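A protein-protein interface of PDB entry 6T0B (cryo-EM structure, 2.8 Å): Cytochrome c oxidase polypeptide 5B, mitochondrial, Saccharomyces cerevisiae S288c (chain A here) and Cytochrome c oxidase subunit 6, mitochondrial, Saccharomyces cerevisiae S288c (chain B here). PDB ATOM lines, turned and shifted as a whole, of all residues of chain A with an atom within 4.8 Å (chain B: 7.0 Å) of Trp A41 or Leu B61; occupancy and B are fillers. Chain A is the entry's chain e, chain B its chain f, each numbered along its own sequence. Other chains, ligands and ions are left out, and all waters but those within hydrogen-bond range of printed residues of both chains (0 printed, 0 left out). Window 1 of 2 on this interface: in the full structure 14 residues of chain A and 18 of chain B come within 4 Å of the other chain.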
ATOM      1  N   GLN A  37     -27.355 -11.091 -21.680  1.00  0.00           N
ATOM      2  CA  GLN A  37     -26.673 -12.333 -21.344  1.00  0.00           C
ATOM      3  C   GLN A  37     -27.513 -13.577 -21.588  1.00  0.00           C
ATOM      4  O   GLN A  37     -26.961 -14.677 -21.572  1.00  0.00           O
ATOM      5  CB  GLN A  37     -26.225 -12.316 -19.893  1.00  0.00           C
ATOM      6  CG  GLN A  37     -24.862 -11.735 -19.687  1.00  0.00           C
ATOM      7  CD  GLN A  37     -24.459 -11.778 -18.249  1.00  0.00           C
ATOM      8  OE1 GLN A  37     -25.113 -12.414 -17.436  1.00  0.00           O
ATOM      9  NE2 GLN A  37     -23.396 -11.077 -17.914  1.00  0.00           N
ATOM     10  N   LEU A  39     -28.714 -14.446 -24.355  1.00  0.00           N
ATOM     11  CA  LEU A  39     -28.394 -14.889 -25.695  1.00  0.00           C
ATOM     12  C   LEU A  39     -27.308 -15.964 -25.651  1.00  0.00           C
ATOM     13  O   LEU A  39     -26.771 -16.272 -24.586  1.00  0.00           O
ATOM     14  CB  LEU A  39     -27.953 -13.685 -26.522  1.00  0.00           C
ATOM     15  CG  LEU A  39     -28.999 -12.596 -26.629  1.00  0.00           C
ATOM     16  CD1 LEU A  39     -28.502 -11.552 -27.578  1.00  0.00           C
ATOM     17  CD2 LEU A  39     -30.318 -13.156 -27.106  1.00  0.00           C
ATOM     18  N   PRO A  40     -26.992 -16.592 -26.784  1.00  0.00           N
ATOM     19  CA  PRO A  40     -25.736 -17.334 -26.860  1.00  0.00           C
ATOM     20  C   PRO A  40     -24.552 -16.409 -26.648  1.00  0.00           C
ATOM     21  O   PRO A  40     -24.563 -15.253 -27.068  1.00  0.00           O
ATOM     22  CB  PRO A  40     -25.759 -17.908 -28.272  1.00  0.00           C
ATOM     23  CG  PRO A  40     -27.168 -18.119 -28.517  1.00  0.00           C
ATOM     24  CD  PRO A  40     -27.883 -16.977 -27.886  1.00  0.00           C
ATOM     25  N   TRP A  41     -23.530 -16.918 -25.975  1.00  0.00           N
ATOM     26  CA  TRP A  41     -22.448 -16.072 -25.511  1.00  0.00           C
ATOM     27  C   TRP A  41     -21.359 -15.878 -26.547  1.00  0.00           C
ATOM     28  O   TRP A  41     -20.317 -15.300 -26.232  1.00  0.00           O
ATOM     29  CB  TRP A  41     -21.865 -16.639 -24.230  1.00  0.00           C
ATOM     30  CG  TRP A  41     -22.809 -16.507 -23.114  1.00  0.00           C
ATOM     31  CD1 TRP A  41     -23.870 -15.668 -23.043  1.00  0.00           C
ATOM     32  CD2 TRP A  41     -22.791 -17.235 -21.895  1.00  0.00           C
ATOM     33  NE1 TRP A  41     -24.519 -15.828 -21.852  1.00  0.00           N
ATOM     34  CE2 TRP A  41     -23.870 -16.788 -21.129  1.00  0.00           C
ATOM     35  CE3 TRP A  41     -21.966 -18.221 -21.376  1.00  0.00           C
ATOM     36  CZ2 TRP A  41     -24.142 -17.296 -19.880  1.00  0.00           C
ATOM     37  CZ3 TRP A  41     -22.234 -18.719 -20.144  1.00  0.00           C
ATOM     38  CH2 TRP A  41     -23.309 -18.262 -19.404  1.00  0.00           C
ATOM     39  N   LYS A  42     -21.568 -16.355 -27.765  1.00  0.00           N
ATOM     40  CA  LYS A  42     -20.726 -15.976 -28.882  1.00  0.00           C
ATOM     41  C   LYS A  42     -21.329 -14.834 -29.682  1.00  0.00           C
ATOM     42  O   LYS A  42     -20.620 -14.196 -30.465  1.00  0.00           O
ATOM     43  CB  LYS A  42     -20.488 -17.184 -29.779  1.00  0.00           C
ATOM     44  CG  LYS A  42     -19.475 -18.137 -29.206  1.00  0.00           C
ATOM     45  CD  LYS A  42     -19.363 -19.404 -30.016  1.00  0.00           C
ATOM     46  CE  LYS A  42     -20.551 -20.291 -29.802  1.00  0.00           C
ATOM     47  NZ  LYS A  42     -20.380 -21.595 -30.486  1.00  0.00           N
ATOM     48  N   THR A  43     -22.621 -14.575 -29.500  1.00  0.00           N
ATOM     49  CA  THR A  43     -23.249 -13.379 -30.041  1.00  0.00           C
ATOM     50  C   THR A  43     -22.690 -12.121 -29.394  1.00  0.00           C
ATOM     51  O   THR A  43     -22.509 -11.103 -30.069  1.00  0.00           O
ATOM     52  CB  THR A  43     -24.761 -13.488 -29.834  1.00  0.00           C
ATOM     53  OG1 THR A  43     -25.271 -14.546 -30.648  1.00  0.00           O
ATOM     54  CG2 THR A  43     -25.501 -12.209 -30.186  1.00  0.00           C
ATOM     55  N   LEU A  44     -22.352 -12.198 -28.112  1.00  0.00           N
ATOM     56  CA  LEU A  44     -21.945 -11.034 -27.341  1.00  0.00           C
ATOM     57  C   LEU A  44     -20.583 -10.533 -27.792  1.00  0.00           C
ATOM     58  O   LEU A  44     -19.664 -11.324 -28.015  1.00  0.00           O
ATOM     59  CB  LEU A  44     -21.898 -11.390 -25.863  1.00  0.00           C
ATOM     60  CG  LEU A  44     -23.142 -11.136 -25.020  1.00  0.00           C
ATOM     61  CD1 LEU A  44     -24.287 -12.040 -25.400  1.00  0.00           C
ATOM     62  CD2 LEU A  44     -22.796 -11.325 -23.574  1.00  0.00           C
ATOM     63  N   ILE A  49     -18.530  -8.054 -22.548  1.00  0.00           N
ATOM     64  CA  ILE A  49     -18.060  -9.063 -21.613  1.00  0.00           C
ATOM     65  C   ILE A  49     -17.152  -8.428 -20.576  1.00  0.00           C
ATOM     66  O   ILE A  49     -17.236  -8.745 -19.384  1.00  0.00           O
ATOM     67  CB  ILE A  49     -17.372 -10.199 -22.377  1.00  0.00           C
ATOM     68  CG1 ILE A  49     -18.333 -10.742 -23.422  1.00  0.00           C
ATOM     69  CG2 ILE A  49     -16.988 -11.297 -21.445  1.00  0.00           C
ATOM     70  CD1 ILE A  49     -17.780 -11.852 -24.235  1.00  0.00           C
ATOM     71  N   LEU B  52     -19.994 -25.120 -15.408  1.00  0.00           N
ATOM     72  CA  LEU B  52     -20.149 -24.300 -16.605  1.00  0.00           C
ATOM     73  C   LEU B  52     -21.545 -24.419 -17.188  1.00  0.00           C
ATOM     74  O   LEU B  52     -22.151 -23.411 -17.569  1.00  0.00           O
ATOM     75  CB  LEU B  52     -19.129 -24.705 -17.656  1.00  0.00           C
ATOM     76  CG  LEU B  52     -17.676 -24.351 -17.406  1.00  0.00           C
ATOM     77  CD1 LEU B  52     -16.832 -25.026 -18.456  1.00  0.00           C
ATOM     78  CD2 LEU B  52     -17.517 -22.866 -17.462  1.00  0.00           C
ATOM     79  N   ALA B  54     -24.198 -25.246 -15.543  1.00  0.00           N
ATOM     80  CA  ALA B  54     -25.111 -24.628 -14.594  1.00  0.00           C
ATOM     81  C   ALA B  54     -25.112 -23.113 -14.722  1.00  0.00           C
ATOM     82  O   ALA B  54     -26.169 -22.485 -14.639  1.00  0.00           O
ATOM     83  CB  ALA B  54     -24.746 -25.041 -13.176  1.00  0.00           C
ATOM     84  N   ALA B  55     -23.945 -22.506 -14.938  1.00  0.00           N
ATOM     85  CA  ALA B  55     -23.919 -21.068 -15.178  1.00  0.00           C
ATOM     86  C   ALA B  55     -24.505 -20.717 -16.533  1.00  0.00           C
ATOM     87  O   ALA B  55     -24.950 -19.583 -16.733  1.00  0.00           O
ATOM     88  CB  ALA B  55     -22.501 -20.526 -15.064  1.00  0.00           C
ATOM     89  N   ARG B  56     -24.509 -21.660 -17.471  1.00  0.00           N
ATOM     90  CA  ARG B  56     -25.226 -21.446 -18.720  1.00  0.00           C
ATOM     91  C   ARG B  56     -26.732 -21.462 -18.505  1.00  0.00           C
ATOM     92  O   ARG B  56     -27.454 -20.676 -19.125  1.00  0.00           O
ATOM     93  CB  ARG B  56     -24.824 -22.504 -19.737  1.00  0.00           C
ATOM     94  CG  ARG B  56     -25.525 -22.402 -21.069  1.00  0.00           C
ATOM     95  CD  ARG B  56     -25.192 -21.115 -21.772  1.00  0.00           C
ATOM     96  NE  ARG B  56     -26.266 -20.141 -21.671  1.00  0.00           N
ATOM     97  CZ  ARG B  56     -26.348 -19.060 -22.425  1.00  0.00           C
ATOM     98  NH1 ARG B  56     -25.426 -18.834 -23.341  1.00  0.00           N
ATOM     99  NH2 ARG B  56     -27.353 -18.219 -22.273  1.00  0.00           N
ATOM    100  N   ARG B  57     -27.224 -22.351 -17.637  1.00  0.00           N
ATOM    101  CA  ARG B  57     -28.663 -22.453 -17.401  1.00  0.00           C
ATOM    102  C   ARG B  57     -29.212 -21.219 -16.726  1.00  0.00           C
ATOM    103  O   ARG B  57     -30.349 -20.821 -16.983  1.00  0.00           O
ATOM    104  CB  ARG B  57     -28.983 -23.645 -16.524  1.00  0.00           C
ATOM    105  CG  ARG B  57     -28.887 -24.983 -17.176  1.00  0.00           C
ATOM    106  CD  ARG B  57     -29.459 -26.040 -16.263  1.00  0.00           C
ATOM    107  NE  ARG B  57     -28.678 -26.232 -15.046  1.00  0.00           N
ATOM    108  CZ  ARG B  57     -29.040 -25.791 -13.849  1.00  0.00           C
ATOM    109  NH1 ARG B  57     -30.164 -25.113 -13.715  1.00  0.00           N
ATOM    110  NH2 ARG B  57     -28.275 -26.005 -12.796  1.00  0.00           N
ATOM    111  N   VAL B  58     -28.439 -20.620 -15.822  1.00  0.00           N
ATOM    112  CA  VAL B  58     -28.882 -19.418 -15.131  1.00  0.00           C
ATOM    113  C   VAL B  58     -28.627 -18.157 -15.957  1.00  0.00           C
ATOM    114  O   VAL B  58     -29.195 -17.092 -15.667  1.00  0.00           O
ATOM    115  CB  VAL B  58     -28.189 -19.440 -13.759  1.00  0.00           C
ATOM    116  CG1 VAL B  58     -28.686 -18.361 -12.886  1.00  0.00           C
ATOM    117  CG2 VAL B  58     -28.479 -20.755 -13.089  1.00  0.00           C
ATOM    118  N   ASN B  59     -27.857 -18.281 -17.037  1.00  0.00           N
ATOM    119  CA  ASN B  59     -27.506 -17.205 -17.959  1.00  0.00           C
ATOM    120  C   ASN B  59     -26.752 -16.085 -17.238  1.00  0.00           C
ATOM    121  O   ASN B  59     -27.227 -14.955 -17.106  1.00  0.00           O
ATOM    122  CB  ASN B  59     -28.736 -16.664 -18.699  1.00  0.00           C
ATOM    123  CG  ASN B  59     -29.536 -17.745 -19.386  1.00  0.00           C
ATOM    124  OD1 ASN B  59     -29.018 -18.513 -20.190  1.00  0.00           O
ATOM    125  ND2 ASN B  59     -30.818 -17.818 -19.055  1.00  0.00           N
ATOM    126  N   ASP B  60     -25.560 -16.434 -16.753  1.00  0.00           N
ATOM    127  CA  ASP B  60     -24.603 -15.466 -16.231  1.00  0.00           C
ATOM    128  C   ASP B  60     -23.234 -15.804 -16.797  1.00  0.00           C
ATOM    129  O   ASP B  60     -22.705 -16.888 -16.559  1.00  0.00           O
ATOM    130  CB  ASP B  60     -24.586 -15.438 -14.700  1.00  0.00           C
ATOM    131  CG  ASP B  60     -23.682 -14.353 -14.140  1.00  0.00           C
ATOM    132  OD1 ASP B  60     -24.237 -13.403 -13.551  1.00  0.00           O
ATOM    133  OD2 ASP B  60     -22.440 -14.472 -14.198  1.00  0.00           O
ATOM    134  N   LEU B  61     -22.663 -14.876 -17.526  1.00  0.00           N
ATOM    135  CA  LEU B  61     -21.381 -15.081 -18.186  1.00  0.00           C
ATOM    136  C   LEU B  61     -20.152 -14.863 -17.299  1.00  0.00           C
ATOM    137  O   LEU B  61     -19.214 -15.659 -17.413  1.00  0.00           O
ATOM    138  CB  LEU B  61     -21.321 -14.205 -19.441  1.00  0.00           C
ATOM    139  CG  LEU B  61     -20.054 -14.129 -20.285  1.00  0.00           C
ATOM    140  CD1 LEU B  61     -19.614 -15.484 -20.739  1.00  0.00           C
ATOM    141  CD2 LEU B  61     -20.314 -13.248 -21.472  1.00  0.00           C
ATOM    142  N   PRO B  62     -20.065 -13.835 -16.433  1.00  0.00           N
ATOM    143  CA  PRO B  62     -18.848 -13.707 -15.624  1.00  0.00           C
ATOM    144  C   PRO B  62     -18.643 -14.793 -14.588  1.00  0.00           C
ATOM    145  O   PRO B  62     -17.505 -14.961 -14.139  1.00  0.00           O
ATOM    146  CB  PRO B  62     -19.019 -12.342 -14.958  1.00  0.00           C
ATOM    147  CG  PRO B  62     -20.414 -12.065 -15.033  1.00  0.00           C
ATOM    148  CD  PRO B  62     -20.828 -12.579 -16.319  1.00  0.00           C
ATOM    149  N   THR B  63     -19.671 -15.544 -14.199  1.00  0.00           N
ATOM    150  CA  THR B  63     -19.425 -16.685 -13.325  1.00  0.00           C
ATOM    151  C   THR B  63     -18.704 -17.803 -14.063  1.00  0.00           C
ATOM    152  O   THR B  63     -17.853 -18.480 -13.478  1.00  0.00           O
ATOM    153  CB  THR B  63     -20.732 -17.184 -12.733  1.00  0.00           C
ATOM    154  OG1 THR B  63     -21.512 -16.062 -12.324  1.00  0.00           O
ATOM    155  CG2 THR B  63     -20.472 -18.050 -11.527  1.00  0.00           C
ATOM    156  N   ALA B  64     -18.974 -17.976 -15.353  1.00  0.00           N
ATOM    157  CA  ALA B  64     -18.251 -18.981 -16.111  1.00  0.00           C
ATOM    158  C   ALA B  64     -16.834 -18.545 -16.455  1.00  0.00           C
ATOM    159  O   ALA B  64     -16.047 -19.365 -16.931  1.00  0.00           O
ATOM    160  CB  ALA B  64     -19.015 -19.333 -17.379  1.00  0.00           C
ATOM    161  N   ILE B  65     -16.493 -17.278 -16.249  1.00  0.00           N
ATOM    162  CA  ILE B  65     -15.107 -16.834 -16.325  1.00  0.00           C
ATOM    163  C   ILE B  65     -14.423 -16.976 -14.979  1.00  0.00           C
ATOM    164  O   ILE B  65     -13.249 -17.359 -14.888  1.00  0.00           O
ATOM    165  CB  ILE B  65     -15.068 -15.380 -16.815  1.00  0.00           C
ATOM    166  CG1 ILE B  65     -15.939 -15.219 -18.047  1.00  0.00           C
ATOM    167  CG2 ILE B  65     -13.661 -14.963 -17.124  1.00  0.00           C
ATOM    168  CD1 ILE B  65     -16.166 -13.798 -18.419  1.00  0.00           C
ATOM    169  N   ARG B  66     -15.166 -16.678 -13.922  1.00  0.00           N
ATOM    170  CA  ARG B  66     -14.643 -16.794 -12.579  1.00  0.00           C
ATOM    171  C   ARG B  66     -14.417 -18.240 -12.180  1.00  0.00           C
ATOM    172  O   ARG B  66     -13.625 -18.489 -11.272  1.00  0.00           O
ATOM    173  CB  ARG B  66     -15.590 -16.110 -11.609  1.00  0.00           C
ATOM    174  CG  ARG B  66     -14.968 -15.701 -10.304  1.00  0.00           C
ATOM    175  CD  ARG B  66     -13.997 -14.571 -10.472  1.00  0.00           C
ATOM    176  NE  ARG B  66     -13.761 -13.913  -9.199  1.00  0.00           N
ATOM    177  CZ  ARG B  66     -13.104 -12.774  -9.056  1.00  0.00           C
ATOM    178  NH1 ARG B  66     -12.605 -12.162 -10.116  1.00  0.00           N
ATOM    179  NH2 ARG B  66     -12.945 -12.249  -7.856  1.00  0.00           N
ATOM    180  N   GLU B  94     -17.540 -24.325 -26.925  1.00  0.00           N
ATOM    181  CA  GLU B  94     -18.929 -24.564 -27.285  1.00  0.00           C
ATOM    182  C   GLU B  94     -19.840 -23.582 -26.578  1.00  0.00           C
ATOM    183  O   GLU B  94     -20.730 -22.988 -27.196  1.00  0.00           O
ATOM    184  CB  GLU B  94     -19.314 -25.994 -26.938  1.00  0.00           C
ATOM    185  CG  GLU B  94     -20.787 -26.239 -26.967  1.00  0.00           C
ATOM    186  CD  GLU B  94     -21.166 -27.495 -26.244  1.00  0.00           C
ATOM    187  OE1 GLU B  94     -20.272 -28.131 -25.653  1.00  0.00           O
ATOM    188  OE2 GLU B  94     -22.362 -27.848 -26.261  1.00  0.00           O
ATOM    189  N   LEU B  95     -19.634 -23.398 -25.278  1.00  0.00           N
ATOM    190  CA  LEU B  95     -20.363 -22.361 -24.565  1.00  0.00           C
ATOM    191  C   LEU B  95     -19.920 -20.976 -24.999  1.00  0.00           C
ATOM    192  O   LEU B  95     -20.722 -20.039 -24.991  1.00  0.00           O
ATOM    193  CB  LEU B  95     -20.172 -22.526 -23.065  1.00  0.00           C
ATOM    194  CG  LEU B  95     -20.944 -23.663 -22.423  1.00  0.00           C
ATOM    195  CD1 LEU B  95     -20.763 -23.618 -20.936  1.00  0.00           C
ATOM    196  CD2 LEU B  95     -22.401 -23.537 -22.773  1.00  0.00           C
ATOM    197  N   GLY B  96     -18.663 -20.828 -25.386  1.00  0.00           N
ATOM    198  CA  GLY B  96     -18.184 -19.552 -25.857  1.00  0.00           C
ATOM    199  C   GLY B  96     -17.832 -18.588 -24.755  1.00  0.00           C
ATOM    200  O   GLY B  96     -18.197 -17.412 -24.830  1.00  0.00           O
ATOM    201  N   VAL B  97     -17.134 -19.049 -23.725  1.00  0.00           N
ATOM    202  CA  VAL B  97     -16.719 -18.147 -22.661  1.00  0.00           C
ATOM    203  C   VAL B  97     -15.239 -17.856 -22.854  1.00  0.00           C
ATOM    204  O   VAL B  97     -14.493 -18.716 -23.343  1.00  0.00           O
ATOM    205  CB  VAL B  97     -17.029 -18.717 -21.267  1.00  0.00           C
ATOM    206  CG1 VAL B  97     -18.499 -18.969 -21.137  1.00  0.00           C
ATOM    207  CG2 VAL B  97     -16.278 -20.002 -20.992  1.00  0.00           C
ATOM    208  N   PRO B  98     -14.791 -16.638 -22.583  1.00  0.00           N
ATOM    209  CA  PRO B  98     -13.364 -16.345 -22.645  1.00  0.00           C
ATOM    210  C   PRO B  98     -12.701 -16.464 -21.289  1.00  0.00           C
ATOM    211  O   PRO B  98     -13.303 -16.232 -20.242  1.00  0.00           O
ATOM    212  CB  PRO B  98     -13.344 -14.896 -23.138  1.00  0.00           C
ATOM    213  CG  PRO B  98     -14.558 -14.325 -22.601  1.00  0.00           C
ATOM    214  CD  PRO B  98     -15.591 -15.407 -22.569  1.00  0.00           C
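The side-chain amide oxygen of Gln A37 lies close to the backbone carbonyl oxygen of Asn B59 (3.3 Å). OE1 of Gln A37 sits at hydrogen-bond distance from N of Leu B61 (3.5 Å). The backbone carbonyl oxygen (O) of Leu A39 sits at hydrogen-bond distance from the guanidinium group (NH2) of Arg B56 (3.1 Å). NE1 of Trp A41 sits close to NH1 of Arg B56 (3.5 Å). O of Trp A41 sits close to O of Gly B96 (3.3 Å).
Among the printed residues, pairs that only touch across the chains: Gln A37 with Arg B56 (3.6 Å), Gln A37 with Asp B60 (3.3 Å), Gln A37 with Pro B62 (3.4 Å), Pro A40 with Arg B56 (3.8 Å), Trp A41 with Ala B55 (3.4 Å), Trp A41 with Asn B59 (3.9 Å), Trp A41 with Asp B60 (3.2 Å), Trp A41 with Leu B61 (3.7 Å), Trp A41 with Leu B95 (3.7 Å), Trp A41 with Val B97 (3.6 Å), Lys A42 with Glu B94 (3.6 Å), Lys A42 with Gly B96 (3.9 Å), Leu A44 with Leu B61 (3.8 Å) and Ile A49 with Leu B61 (3.7 Å).
Of chain B, only Ala B55 (3.4 Å), Arg B56 (3.4 Å), Asn B59 (3.9 Å), Asp B60 (3.2 Å), Leu B61 (3.7 Å), Leu B95 (3.7 Å), Gly B96 (3.3 Å) and Val B97 (3.6 Å) come within 4 Å of Trp A41. Leu B61 touches just these residues of chain A: Gln A37, Trp A41, Leu A44 and Ile A49. Of the printed residues of chain B, Pro A40 touches Arg B56. Of the printed residues of chain A, Leu B95 touches Trp A41. Of the printed residues of chain A, Gly B96 touches Trp A41 (3.3 Å) and Lys A42 (3.9 Å). Of the printed residues of chain A, Asp B60 touches Gln A37 (3.3 Å) and Trp A41 (3.2 Å). Printed residues of chain A within 4 Å of Asn B59: Gln A37 (3.3 Å) and Trp A41 (3.9 Å). The nearest residue of chain B that does not touch Trp A41 is Ala B64 (4.3 Å). The nearest printed residue of chain A that does not touch Leu B61 is Lys A42 (7.1 Å).
O of Gln A37 lies within hydrogen-bond range of NE1 of Trp A41, at 2.7 Å. The backbone NH (N) of Asp B60 lies within hydrogen-bond range of the backbone carbonyl oxygen (O) of Ala B55 (3.2 Å). OD1 of Asn B59 lies within hydrogen-bond range of NH2 of Arg B56 (2.7 Å). The side-chain hydroxyl (OG1) of Thr B63 sits at hydrogen-bond distance from the side-chain carboxylate (OD2) of Asp B60.
Hydrophobic or aromatic side chains of chain B that line the printed part of chain A: Leu B61, Pro B62 and Val B97. Of the 8 printed residues of chain A, 7 touch a printed residue of chain B. Printed residues of chain A that touch a printed residue of chain B: Gln A37, Leu A39, Pro A40, Trp A41, Lys A42, Leu A44 and Ile A49. Hydrophobic or aromatic side chains of chain A that line the printed part of chain B: Trp A41, Leu A44 and Ile A49. Among the printed residues, 19 pairs touch across the chains. Among the printed residues, no Asp or Glu carboxylate lies within 4 Å of a Lys or Arg side-chain nitrogen of the other chain.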
